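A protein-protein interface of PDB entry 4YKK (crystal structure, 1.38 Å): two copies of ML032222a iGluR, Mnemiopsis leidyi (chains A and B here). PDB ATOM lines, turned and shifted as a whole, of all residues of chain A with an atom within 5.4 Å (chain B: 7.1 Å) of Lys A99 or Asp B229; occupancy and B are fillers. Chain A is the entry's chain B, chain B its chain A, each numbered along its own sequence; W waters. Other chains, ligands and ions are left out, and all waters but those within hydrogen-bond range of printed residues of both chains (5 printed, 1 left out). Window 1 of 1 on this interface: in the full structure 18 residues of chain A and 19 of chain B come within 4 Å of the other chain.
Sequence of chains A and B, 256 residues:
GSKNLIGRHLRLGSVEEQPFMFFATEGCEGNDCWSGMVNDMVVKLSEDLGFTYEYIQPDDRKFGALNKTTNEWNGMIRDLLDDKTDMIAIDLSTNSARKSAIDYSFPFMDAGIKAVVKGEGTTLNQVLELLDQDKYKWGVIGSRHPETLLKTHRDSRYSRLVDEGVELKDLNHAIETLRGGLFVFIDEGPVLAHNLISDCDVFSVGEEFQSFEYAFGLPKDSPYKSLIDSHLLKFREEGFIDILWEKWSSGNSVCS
Of the printed residues of chain B, Asn A95 touches Leu B233 (3.7 Å).
Printed residues of chain B within 4 Å of Ser A96: Lys B234 (3.7 Å).
Printed residues of chain B within 4 Å of Lys A99: Ser B226 (3.5 Å), Asp B229 (3.7 Å), Ser B230 (2.9 Å) and Leu B233 (3.6 Å).
Ala A101 touches none of the printed residues of chain B.
Asp A103 touches none of the printed residues of chain B.
Asn A95 touches Leu B233 (O to CD2, 3.7 Å).
OG of Ser A96 touches CA of Lys B234, at 3.7 Å.
Lys A99 touches Asp B229.
Lys A99 touches Leu B233.
1 position is printed for both chains.
Of the 6 pairs that touch across the chains among the printed residues, none has its exchanged pair printed and touching as well.
The backbone carbonyl oxygen of Ser B226 lies within hydrogen-bond range of the side-chain amino group of Lys A99, 3.5 Å away.
OG of Ser B230 sits at hydrogen-bond distance from NZ of Lys A99 (2.9 Å).
Water W5 lies within hydrogen-bond range of the side-chain carboxylate (OD2) of Asp B229 (2.7 Å) and the side-chain amino group (NZ) of Lys A99 (3.3 Å).
Water W1 bridges the side-chain carboxylate of Asp A103 (2.7 Å) and the side-chain hydroxyl of Ser B226 (2.8 Å).
Water W2 lies within hydrogen-bond range of O of Lys A99 (2.7 Å), NZ of Lys A220 (2.9 Å) and OG of Ser B230 (3.2 Å).
Water W4 bridges the backbone carbonyl oxygen of Ser B230 (2.8 Å) and the side-chain hydroxyl of Ser A96 (2.8 Å).
Water W3 lies within hydrogen-bond range of O of Tyr A104, NZ of Lys B225 and OD2 of Asp B229.
The side-chain hydroxyl (OG) of Ser B230 is in hydrogen-bond range of the backbone carbonyl oxygen (O) of Ser B226, 3.3 Å away.
The side-chain amide oxygen (OD1) of Asn A95 sits at hydrogen-bond distance from the backbone NH (N) of Ala A97, at 3.2 Å.
OH of Tyr A104 lies within hydrogen-bond range of N of Asn A95, at 3.1 Å.
The side-chain amide oxygen of Asn A95 is in hydrogen-bond range of the backbone NH of Arg A98 (2.9 Å).
OD1 of Asp B229 sits at hydrogen-bond distance from N of Phe B106 (2.8 Å).
The side-chain amino group of Lys B225 lies within salt-bridge range of the side-chain carboxylate of Asp B229 (2.7 Å).
Of the 19 printed residues of chain B, 5 touch a printed residue of chain A.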
ATOM      1  N   ASN A  95      34.488  10.797  -7.420  1.00  0.00           N
ATOM      2  CA  ASN A  95      34.252  12.237  -7.643  1.00  0.00           C
ATOM      3  C   ASN A  95      32.946  12.457  -8.381  1.00  0.00           C
ATOM      4  O   ASN A  95      32.421  11.554  -9.030  1.00  0.00           O
ATOM      5  CB  ASN A  95      35.469  12.980  -8.246  1.00  0.00           C
ATOM      6  CG  ASN A  95      35.790  12.611  -9.679  1.00  0.00           C
ATOM      7  OD1 ASN A  95      34.923  12.660 -10.564  1.00  0.00           O
ATOM      8  ND2 ASN A  95      37.055  12.336  -9.939  1.00  0.00           N
ATOM      9  N   SER A  96      32.392  13.659  -8.236  1.00  0.00           N
ATOM     10  CA  SER A  96      31.094  13.967  -8.806  1.00  0.00           C
ATOM     11  C   SER A  96      31.084  13.948 -10.328  1.00  0.00           C
ATOM     12  O   SER A  96      30.098  13.562 -10.932  1.00  0.00           O
ATOM     13  CB  SER A  96      30.583  15.310  -8.295  1.00  0.00           C
ATOM     14  OG  SER A  96      30.272  15.227  -6.913  1.00  0.00           O
ATOM     15  N   ALA A  97      32.181  14.347 -10.955  1.00  0.00           N
ATOM     16  CA  ALA A  97      32.225  14.311 -12.408  1.00  0.00           C
ATOM     17  C   ALA A  97      32.024  12.880 -12.909  1.00  0.00           C
ATOM     18  O   ALA A  97      31.187  12.596 -13.758  1.00  0.00           O
ATOM     19  CB  ALA A  97      33.531  14.882 -12.911  1.00  0.00           C
ATOM     20  N   ARG A  98      32.772  11.935 -12.348  1.00  0.00           N
ATOM     21  CA  ARG A  98      32.636  10.532 -12.728  1.00  0.00           C
ATOM     22  C   ARG A  98      31.257   9.988 -12.396  1.00  0.00           C
ATOM     23  O   ARG A  98      30.680   9.253 -13.190  1.00  0.00           O
ATOM     24  CB  ARG A  98      33.710   9.690 -12.059  1.00  0.00           C
ATOM     25  CG  ARG A  98      35.110   9.934 -12.645  1.00  0.00           C
ATOM     26  CD  ARG A  98      36.195   9.321 -11.798  1.00  0.00           C
ATOM     27  NE  ARG A  98      37.509   9.475 -12.414  1.00  0.00           N
ATOM     28  CZ  ARG A  98      38.647   9.149 -11.828  1.00  0.00           C
ATOM     29  NH1 ARG A  98      38.649   8.657 -10.599  1.00  0.00           N
ATOM     30  NH2 ARG A  98      39.794   9.319 -12.472  1.00  0.00           N
ATOM     31  N   LYS A  99      30.731  10.370 -11.233  1.00  0.00           N
ATOM     32  CA  LYS A  99      29.440   9.873 -10.776  1.00  0.00           C
ATOM     33  C   LYS A  99      28.300  10.303 -11.711  1.00  0.00           C
ATOM     34  O   LYS A  99      27.252   9.667 -11.746  1.00  0.00           O
ATOM     35  CB  LYS A  99      29.202  10.373  -9.348  1.00  0.00           C
ATOM     36  CG  LYS A  99      27.877   9.972  -8.691  1.00  0.00           C
ATOM     37  CD  LYS A  99      27.793   8.473  -8.384  1.00  0.00           C
ATOM     38  CE  LYS A  99      26.491   8.121  -7.673  1.00  0.00           C
ATOM     39  NZ  LYS A  99      25.299   8.201  -8.566  1.00  0.00           N
ATOM     40  N   SER A 100      28.513  11.367 -12.487  1.00  0.00           N
ATOM     41  CA  SER A 100      27.512  11.778 -13.469  1.00  0.00           C
ATOM     42  C   SER A 100      27.412  10.770 -14.618  1.00  0.00           C
ATOM     43  O   SER A 100      26.362  10.636 -15.245  1.00  0.00           O
ATOM     44  CB  SER A 100      27.782  13.190 -14.014  1.00  0.00           C
ATOM     45  OG  SER A 100      28.923  13.254 -14.870  1.00  0.00           O
ATOM     46  N   ALA A 101      28.513  10.071 -14.888  1.00  0.00           N
ATOM     47  CA  ALA A 101      28.604   9.132 -16.018  1.00  0.00           C
ATOM     48  C   ALA A 101      28.571   7.654 -15.658  1.00  0.00           C
ATOM     49  O   ALA A 101      28.048   6.869 -16.445  1.00  0.00           O
ATOM     50  CB  ALA A 101      29.856   9.432 -16.826  1.00  0.00           C
ATOM     51  N   ILE A 102      29.122   7.276 -14.505  1.00  0.00           N
ATOM     52  CA  ILE A 102      29.213   5.884 -14.069  1.00  0.00           C
ATOM     53  C   ILE A 102      28.769   5.743 -12.629  1.00  0.00           C
ATOM     54  O   ILE A 102      28.552   6.745 -11.940  1.00  0.00           O
ATOM     55  CB  ILE A 102      30.681   5.347 -14.201  1.00  0.00           C
ATOM     56  CG1 ILE A 102      31.640   6.080 -13.259  1.00  0.00           C
ATOM     57  CG2 ILE A 102      31.182   5.462 -15.631  1.00  0.00           C
ATOM     58  CD1 ILE A 102      32.895   5.249 -12.949  1.00  0.00           C
ATOM     59  N   ASP A 103      28.630   4.500 -12.184  1.00  0.00           N
ATOM     60  CA  ASP A 103      28.385   4.195 -10.797  1.00  0.00           C
ATOM     61  C   ASP A 103      29.688   3.710 -10.155  1.00  0.00           C
ATOM     62  O   ASP A 103      30.672   3.365 -10.830  1.00  0.00           O
ATOM     63  CB  ASP A 103      27.305   3.109 -10.628  1.00  0.00           C
ATOM     64  CG  ASP A 103      25.885   3.623 -10.836  1.00  0.00           C
ATOM     65  OD1 ASP A 103      25.670   4.857 -10.894  1.00  0.00           O
ATOM     66  OD2 ASP A 103      24.984   2.753 -10.937  1.00  0.00           O
ATOM     67  N   TYR A 104      29.662   3.676  -8.832  1.00  0.00           N
ATOM     68  CA  TYR A 104      30.744   3.134  -8.036  1.00  0.00           C
ATOM     69  C   TYR A 104      30.243   1.955  -7.248  1.00  0.00           C
ATOM     70  O   TYR A 104      29.081   1.925  -6.814  1.00  0.00           O
ATOM     71  CB  TYR A 104      31.275   4.176  -7.075  1.00  0.00           C
ATOM     72  CG  TYR A 104      32.090   5.271  -7.717  1.00  0.00           C
ATOM     73  CD1 TYR A 104      33.440   5.064  -8.020  1.00  0.00           C
ATOM     74  CD2 TYR A 104      31.531   6.504  -7.981  1.00  0.00           C
ATOM     75  CE1 TYR A 104      34.196   6.059  -8.568  1.00  0.00           C
ATOM     76  CE2 TYR A 104      32.279   7.516  -8.549  1.00  0.00           C
ATOM     77  CZ  TYR A 104      33.610   7.278  -8.831  1.00  0.00           C
ATOM     78  OH  TYR A 104      34.364   8.316  -9.326  1.00  0.00           O
ATOM     79  N   LYS A 220      26.355   2.393 -15.319  1.00  0.00           N
ATOM     80  CA  LYS A 220      24.992   2.546 -14.844  1.00  0.00           C
ATOM     81  C   LYS A 220      24.173   1.370 -15.356  1.00  0.00           C
ATOM     82  O   LYS A 220      24.409   0.860 -16.462  1.00  0.00           O
ATOM     83  CB  LYS A 220      24.417   3.879 -15.303  1.00  0.00           C
ATOM     84  CG  LYS A 220      25.089   5.078 -14.635  1.00  0.00           C
ATOM     85  CD  LYS A 220      24.477   6.369 -15.086  1.00  0.00           C
ATOM     86  CE  LYS A 220      25.017   7.488 -14.239  1.00  0.00           C
ATOM     87  NZ  LYS A 220      24.214   8.746 -14.307  1.00  0.00           N
ATOM     88  N   LEU B  45      18.919  18.098   0.909  1.00  0.00           N
ATOM     89  CA  LEU B  45      18.446  17.193  -0.141  1.00  0.00           C
ATOM     90  C   LEU B  45      17.050  17.573  -0.648  1.00  0.00           C
ATOM     91  O   LEU B  45      16.792  17.578  -1.850  1.00  0.00           O
ATOM     92  CB  LEU B  45      18.429  15.746   0.345  1.00  0.00           C
ATOM     93  CG  LEU B  45      19.795  15.066   0.530  1.00  0.00           C
ATOM     94  CD1 LEU B  45      19.608  13.771   1.302  1.00  0.00           C
ATOM     95  CD2 LEU B  45      20.506  14.832  -0.821  1.00  0.00           C
ATOM     96  N   TYR B 104      22.302   0.322   0.704  1.00  0.00           N
ATOM     97  CA  TYR B 104      22.812   1.516   1.346  1.00  0.00           C
ATOM     98  C   TYR B 104      23.069   2.572   0.300  1.00  0.00           C
ATOM     99  O   TYR B 104      23.423   2.276  -0.851  1.00  0.00           O
ATOM    100  CB  TYR B 104      24.115   1.220   2.053  1.00  0.00           C
ATOM    101  CG  TYR B 104      23.990   0.387   3.303  1.00  0.00           C
ATOM    102  CD1 TYR B 104      23.633   0.971   4.511  1.00  0.00           C
ATOM    103  CD2 TYR B 104      24.255  -0.958   3.294  1.00  0.00           C
ATOM    104  CE1 TYR B 104      23.557   0.241   5.665  1.00  0.00           C
ATOM    105  CE2 TYR B 104      24.161  -1.713   4.468  1.00  0.00           C
ATOM    106  CZ  TYR B 104      23.820  -1.102   5.640  1.00  0.00           C
ATOM    107  OH  TYR B 104      23.768  -1.836   6.810  1.00  0.00           O
ATOM    108  N   SER B 105      22.896   3.826   0.704  1.00  0.00           N
ATOM    109  CA  SER B 105      23.353   4.937  -0.102  1.00  0.00           C
ATOM    110  C   SER B 105      24.874   5.015  -0.089  1.00  0.00           C
ATOM    111  O   SER B 105      25.543   4.298   0.669  1.00  0.00           O
ATOM    112  CB  SER B 105      22.821   6.246   0.463  1.00  0.00           C
ATOM    113  OG  SER B 105      23.486   6.584   1.679  1.00  0.00           O
ATOM    114  N   PHE B 106      25.398   5.935  -0.892  1.00  0.00           N
ATOM    115  CA  PHE B 106      26.780   6.364  -0.749  1.00  0.00           C
ATOM    116  C   PHE B 106      27.020   6.768   0.700  1.00  0.00           C
ATOM    117  O   PHE B 106      26.153   7.374   1.322  1.00  0.00           O
ATOM    118  CB  PHE B 106      27.043   7.541  -1.698  1.00  0.00           C
ATOM    119  CG  PHE B 106      28.498   7.825  -1.900  1.00  0.00           C
ATOM    120  CD1 PHE B 106      29.238   7.083  -2.803  1.00  0.00           C
ATOM    121  CD2 PHE B 106      29.134   8.799  -1.166  1.00  0.00           C
ATOM    122  CE1 PHE B 106      30.598   7.316  -2.978  1.00  0.00           C
ATOM    123  CE2 PHE B 106      30.497   9.021  -1.316  1.00  0.00           C
ATOM    124  CZ  PHE B 106      31.219   8.283  -2.226  1.00  0.00           C
ATOM    125  N   PRO B 107      28.165   6.373   1.286  1.00  0.00           N
ATOM    126  CA  PRO B 107      28.366   6.676   2.701  1.00  0.00           C
ATOM    127  C   PRO B 107      28.691   8.138   2.979  1.00  0.00           C
ATOM    128  O   PRO B 107      29.226   8.824   2.094  1.00  0.00           O
ATOM    129  CB  PRO B 107      29.562   5.804   3.078  1.00  0.00           C
ATOM    130  CG  PRO B 107      30.300   5.610   1.811  1.00  0.00           C
ATOM    131  CD  PRO B 107      29.251   5.540   0.745  1.00  0.00           C
ATOM    132  N   PHE B 216      22.747   6.112   4.440  1.00  0.00           N
ATOM    133  CA  PHE B 216      21.294   5.980   4.534  1.00  0.00           C
ATOM    134  C   PHE B 216      20.883   4.591   4.026  1.00  0.00           C
ATOM    135  O   PHE B 216      21.608   3.962   3.267  1.00  0.00           O
ATOM    136  CB  PHE B 216      20.589   7.063   3.708  1.00  0.00           C
ATOM    137  CG  PHE B 216      20.685   8.471   4.280  1.00  0.00           C
ATOM    138  CD1 PHE B 216      21.256   8.723   5.522  1.00  0.00           C
ATOM    139  CD2 PHE B 216      20.202   9.544   3.555  1.00  0.00           C
ATOM    140  CE1 PHE B 216      21.315  10.026   6.019  1.00  0.00           C
ATOM    141  CE2 PHE B 216      20.267  10.838   4.046  1.00  0.00           C
ATOM    142  CZ  PHE B 216      20.845  11.080   5.275  1.00  0.00           C
ATOM    143  N   LEU B 218      18.225   2.155   1.932  1.00  0.00           N
ATOM    144  CA  LEU B 218      17.279   2.226   0.829  1.00  0.00           C
ATOM    145  C   LEU B 218      16.729   0.839   0.541  1.00  0.00           C
ATOM    146  O   LEU B 218      17.451  -0.158   0.658  1.00  0.00           O
ATOM    147  CB  LEU B 218      17.977   2.782  -0.428  1.00  0.00           C
ATOM    148  CG  LEU B 218      18.299   4.283  -0.370  1.00  0.00           C
ATOM    149  CD1 LEU B 218      19.431   4.622  -1.346  1.00  0.00           C
ATOM    150  CD2 LEU B 218      17.070   5.087  -0.669  1.00  0.00           C
ATOM    151  N   TYR B 224      15.026   5.932  -6.231  1.00  0.00           N
ATOM    152  CA  TYR B 224      15.663   7.161  -5.745  1.00  0.00           C
ATOM    153  C   TYR B 224      17.153   6.998  -5.413  1.00  0.00           C
ATOM    154  O   TYR B 224      17.841   7.977  -5.102  1.00  0.00           O
ATOM    155  CB  TYR B 224      14.918   7.677  -4.509  1.00  0.00           C
ATOM    156  CG  TYR B 224      13.428   7.815  -4.734  1.00  0.00           C
ATOM    157  CD1 TYR B 224      12.938   8.398  -5.894  1.00  0.00           C
ATOM    158  CD2 TYR B 224      12.518   7.329  -3.809  1.00  0.00           C
ATOM    159  CE1 TYR B 224      11.571   8.519  -6.120  1.00  0.00           C
ATOM    160  CE2 TYR B 224      11.139   7.448  -4.021  1.00  0.00           C
ATOM    161  CZ  TYR B 224      10.684   8.037  -5.180  1.00  0.00           C
ATOM    162  OH  TYR B 224       9.326   8.160  -5.400  1.00  0.00           O
ATOM    163  N   LYS B 225      17.672   5.778  -5.480  1.00  0.00           N
ATOM    164  CA  LYS B 225      19.037   5.550  -4.998  1.00  0.00           C
ATOM    165  C   LYS B 225      20.083   6.349  -5.772  1.00  0.00           C
ATOM    166  O   LYS B 225      20.986   6.936  -5.171  1.00  0.00           O
ATOM    167  CB  LYS B 225      19.410   4.072  -5.019  1.00  0.00           C
ATOM    168  CG  LYS B 225      20.866   3.824  -4.607  1.00  0.00           C
ATOM    169  CD  LYS B 225      21.164   2.359  -4.351  1.00  0.00           C
ATOM    170  CE  LYS B 225      22.653   2.026  -4.488  1.00  0.00           C
ATOM    171  NZ  LYS B 225      23.546   2.747  -3.552  1.00  0.00           N
ATOM    172  N   SER B 226      19.965   6.371  -7.093  1.00  0.00           N
ATOM    173  CA  SER B 226      20.949   7.056  -7.925  1.00  0.00           C
ATOM    174  C   SER B 226      21.075   8.517  -7.513  1.00  0.00           C
ATOM    175  O   SER B 226      22.187   9.024  -7.284  1.00  0.00           O
ATOM    176  CB  SER B 226      20.550   6.972  -9.398  1.00  0.00           C
ATOM    177  OG  SER B 226      21.387   7.791 -10.200  1.00  0.00           O
ATOM    178  N   LEU B 227      19.942   9.208  -7.432  1.00  0.00           N
ATOM    179  CA  LEU B 227      19.943  10.624  -7.080  1.00  0.00           C
ATOM    180  C   LEU B 227      20.425  10.870  -5.653  1.00  0.00           C
ATOM    181  O   LEU B 227      21.196  11.792  -5.392  1.00  0.00           O
ATOM    182  CB  LEU B 227      18.554  11.251  -7.278  1.00  0.00           C
ATOM    183  CG  LEU B 227      18.213  11.656  -8.713  1.00  0.00           C
ATOM    184  CD1 LEU B 227      16.744  12.054  -8.785  1.00  0.00           C
ATOM    185  CD2 LEU B 227      19.090  12.794  -9.161  1.00  0.00           C
ATOM    186  N   ILE B 228      19.984  10.057  -4.706  1.00  0.00           N
ATOM    187  CA  ILE B 228      20.444  10.239  -3.347  1.00  0.00           C
ATOM    188  C   ILE B 228      21.961  10.041  -3.302  1.00  0.00           C
ATOM    189  O   ILE B 228      22.686  10.851  -2.709  1.00  0.00           O
ATOM    190  CB  ILE B 228      19.716   9.283  -2.354  1.00  0.00           C
ATOM    191  CG1 ILE B 228      18.219   9.627  -2.262  1.00  0.00           C
ATOM    192  CG2 ILE B 228      20.357   9.334  -0.964  1.00  0.00           C
ATOM    193  CD1 ILE B 228      17.908  10.989  -1.723  1.00  0.00           C
ATOM    194  N   ASP B 229      22.452   9.012  -3.980  1.00  0.00           N
ATOM    195  CA  ASP B 229      23.895   8.730  -3.953  1.00  0.00           C
ATOM    196  C   ASP B 229      24.696   9.890  -4.541  1.00  0.00           C
ATOM    197  O   ASP B 229      25.709  10.305  -3.986  1.00  0.00           O
ATOM    198  CB  ASP B 229      24.229   7.486  -4.769  1.00  0.00           C
ATOM    199  CG  ASP B 229      23.843   6.187  -4.090  1.00  0.00           C
ATOM    200  OD1 ASP B 229      23.413   6.216  -2.912  1.00  0.00           O
ATOM    201  OD2 ASP B 229      23.972   5.130  -4.747  1.00  0.00           O
ATOM    202  N   SER B 230      24.253  10.387  -5.686  1.00  0.00           N
ATOM    203  CA  SER B 230      24.939  11.488  -6.342  1.00  0.00           C
ATOM    204  C   SER B 230      25.030  12.705  -5.431  1.00  0.00           C
ATOM    205  O   SER B 230      26.084  13.319  -5.274  1.00  0.00           O
ATOM    206  CB  SER B 230      24.220  11.867  -7.633  1.00  0.00           C
ATOM    207  OG  SER B 230      24.481  10.938  -8.674  1.00  0.00           O
ATOM    208  N   HIS B 231      23.915  13.043  -4.797  1.00  0.00           N
ATOM    209  CA  HIS B 231      23.874  14.231  -3.976  1.00  0.00           C
ATOM    210  C   HIS B 231      24.662  14.051  -2.683  1.00  0.00           C
ATOM    211  O   HIS B 231      25.332  14.977  -2.227  1.00  0.00           O
ATOM    212  CB  HIS B 231      22.432  14.681  -3.750  1.00  0.00           C
ATOM    213  CG  HIS B 231      21.846  15.323  -4.964  1.00  0.00           C
ATOM    214  ND1 HIS B 231      21.630  16.681  -5.059  1.00  0.00           N
ATOM    215  CD2 HIS B 231      21.493  14.800  -6.160  1.00  0.00           C
ATOM    216  CE1 HIS B 231      21.147  16.964  -6.258  1.00  0.00           C
ATOM    217  NE2 HIS B 231      21.057  15.843  -6.947  1.00  0.00           N
ATOM    218  N   LEU B 232      24.673  12.849  -2.113  1.00  0.00           N
ATOM    219  CA  LEU B 232      25.491  12.628  -0.939  1.00  0.00           C
ATOM    220  C   LEU B 232      26.977  12.701  -1.280  1.00  0.00           C
ATOM    221  O   LEU B 232      27.766  13.223  -0.502  1.00  0.00           O
ATOM    222  CB  LEU B 232      25.155  11.306  -0.274  1.00  0.00           C
ATOM    223  CG  LEU B 232      23.828  11.259   0.470  1.00  0.00           C
ATOM    224  CD1 LEU B 232      23.577   9.825   0.932  1.00  0.00           C
ATOM    225  CD2 LEU B 232      23.806  12.238   1.607  1.00  0.00           C
ATOM    226  N   LEU B 233      27.365  12.176  -2.429  1.00  0.00           N
ATOM    227  CA  LEU B 233      28.757  12.291  -2.859  1.00  0.00           C
ATOM    228  C   LEU B 233      29.138  13.771  -2.998  1.00  0.00           C
ATOM    229  O   LEU B 233      30.209  14.194  -2.547  1.00  0.00           O
ATOM    230  CB  LEU B 233      28.982  11.534  -4.165  1.00  0.00           C
ATOM    231  CG  LEU B 233      30.364  11.657  -4.809  1.00  0.00           C
ATOM    232  CD1 LEU B 233      31.482  11.364  -3.851  1.00  0.00           C
ATOM    233  CD2 LEU B 233      30.432  10.727  -6.003  1.00  0.00           C
ATOM    234  N   LYS B 234      28.267  14.561  -3.612  1.00  0.00           N
ATOM    235  CA  LYS B 234      28.530  15.979  -3.757  1.00  0.00           C
ATOM    236  C   LYS B 234      28.661  16.664  -2.403  1.00  0.00           C
ATOM    237  O   LYS B 234      29.512  17.515  -2.221  1.00  0.00           O
ATOM    238  CB  LYS B 234      27.432  16.629  -4.602  1.00  0.00           C
ATOM    239  CG  LYS B 234      27.616  18.113  -4.905  1.00  0.00           C
ATOM    240  CD  LYS B 234      26.484  18.576  -5.829  1.00  0.00           C
ATOM    241  CE  LYS B 234      26.528  20.065  -6.131  1.00  0.00           C
ATOM    242  NZ  LYS B 234      25.391  20.493  -6.991  1.00  0.00           N
ATOM    243  N   PHE B 235      27.825  16.291  -1.441  1.00  0.00           N
ATOM    244  CA  PHE B 235      27.935  16.856  -0.094  1.00  0.00           C
ATOM    245  C   PHE B 235      29.337  16.589   0.452  1.00  0.00           C
ATOM    246  O   PHE B 235      29.952  17.461   1.069  1.00  0.00           O
ATOM    247  CB  PHE B 235      26.945  16.212   0.887  1.00  0.00           C
ATOM    248  CG  PHE B 235      25.508  16.678   0.757  1.00  0.00           C
ATOM    249  CD1 PHE B 235      25.108  17.695  -0.092  1.00  0.00           C
ATOM    250  CD2 PHE B 235      24.545  16.056   1.532  1.00  0.00           C
ATOM    251  CE1 PHE B 235      23.770  18.082  -0.149  1.00  0.00           C
ATOM    252  CE2 PHE B 235      23.226  16.446   1.484  1.00  0.00           C
ATOM    253  CZ  PHE B 235      22.829  17.438   0.635  1.00  0.00           C
HETATM  254  O   HOH W   1      23.168   5.912 -11.278  1.00  0.00           O
HETATM  255  O   HOH W   2      24.520   9.952 -11.680  1.00  0.00           O
HETATM  256  O   HOH W   3      26.724   3.112  -4.695  1.00  0.00           O
HETATM  257  O   HOH W   4      28.084  13.456  -7.262  1.00  0.00           O
HETATM  258  O   HOH W   5      24.467   5.277  -7.368  1.00  0.00           O
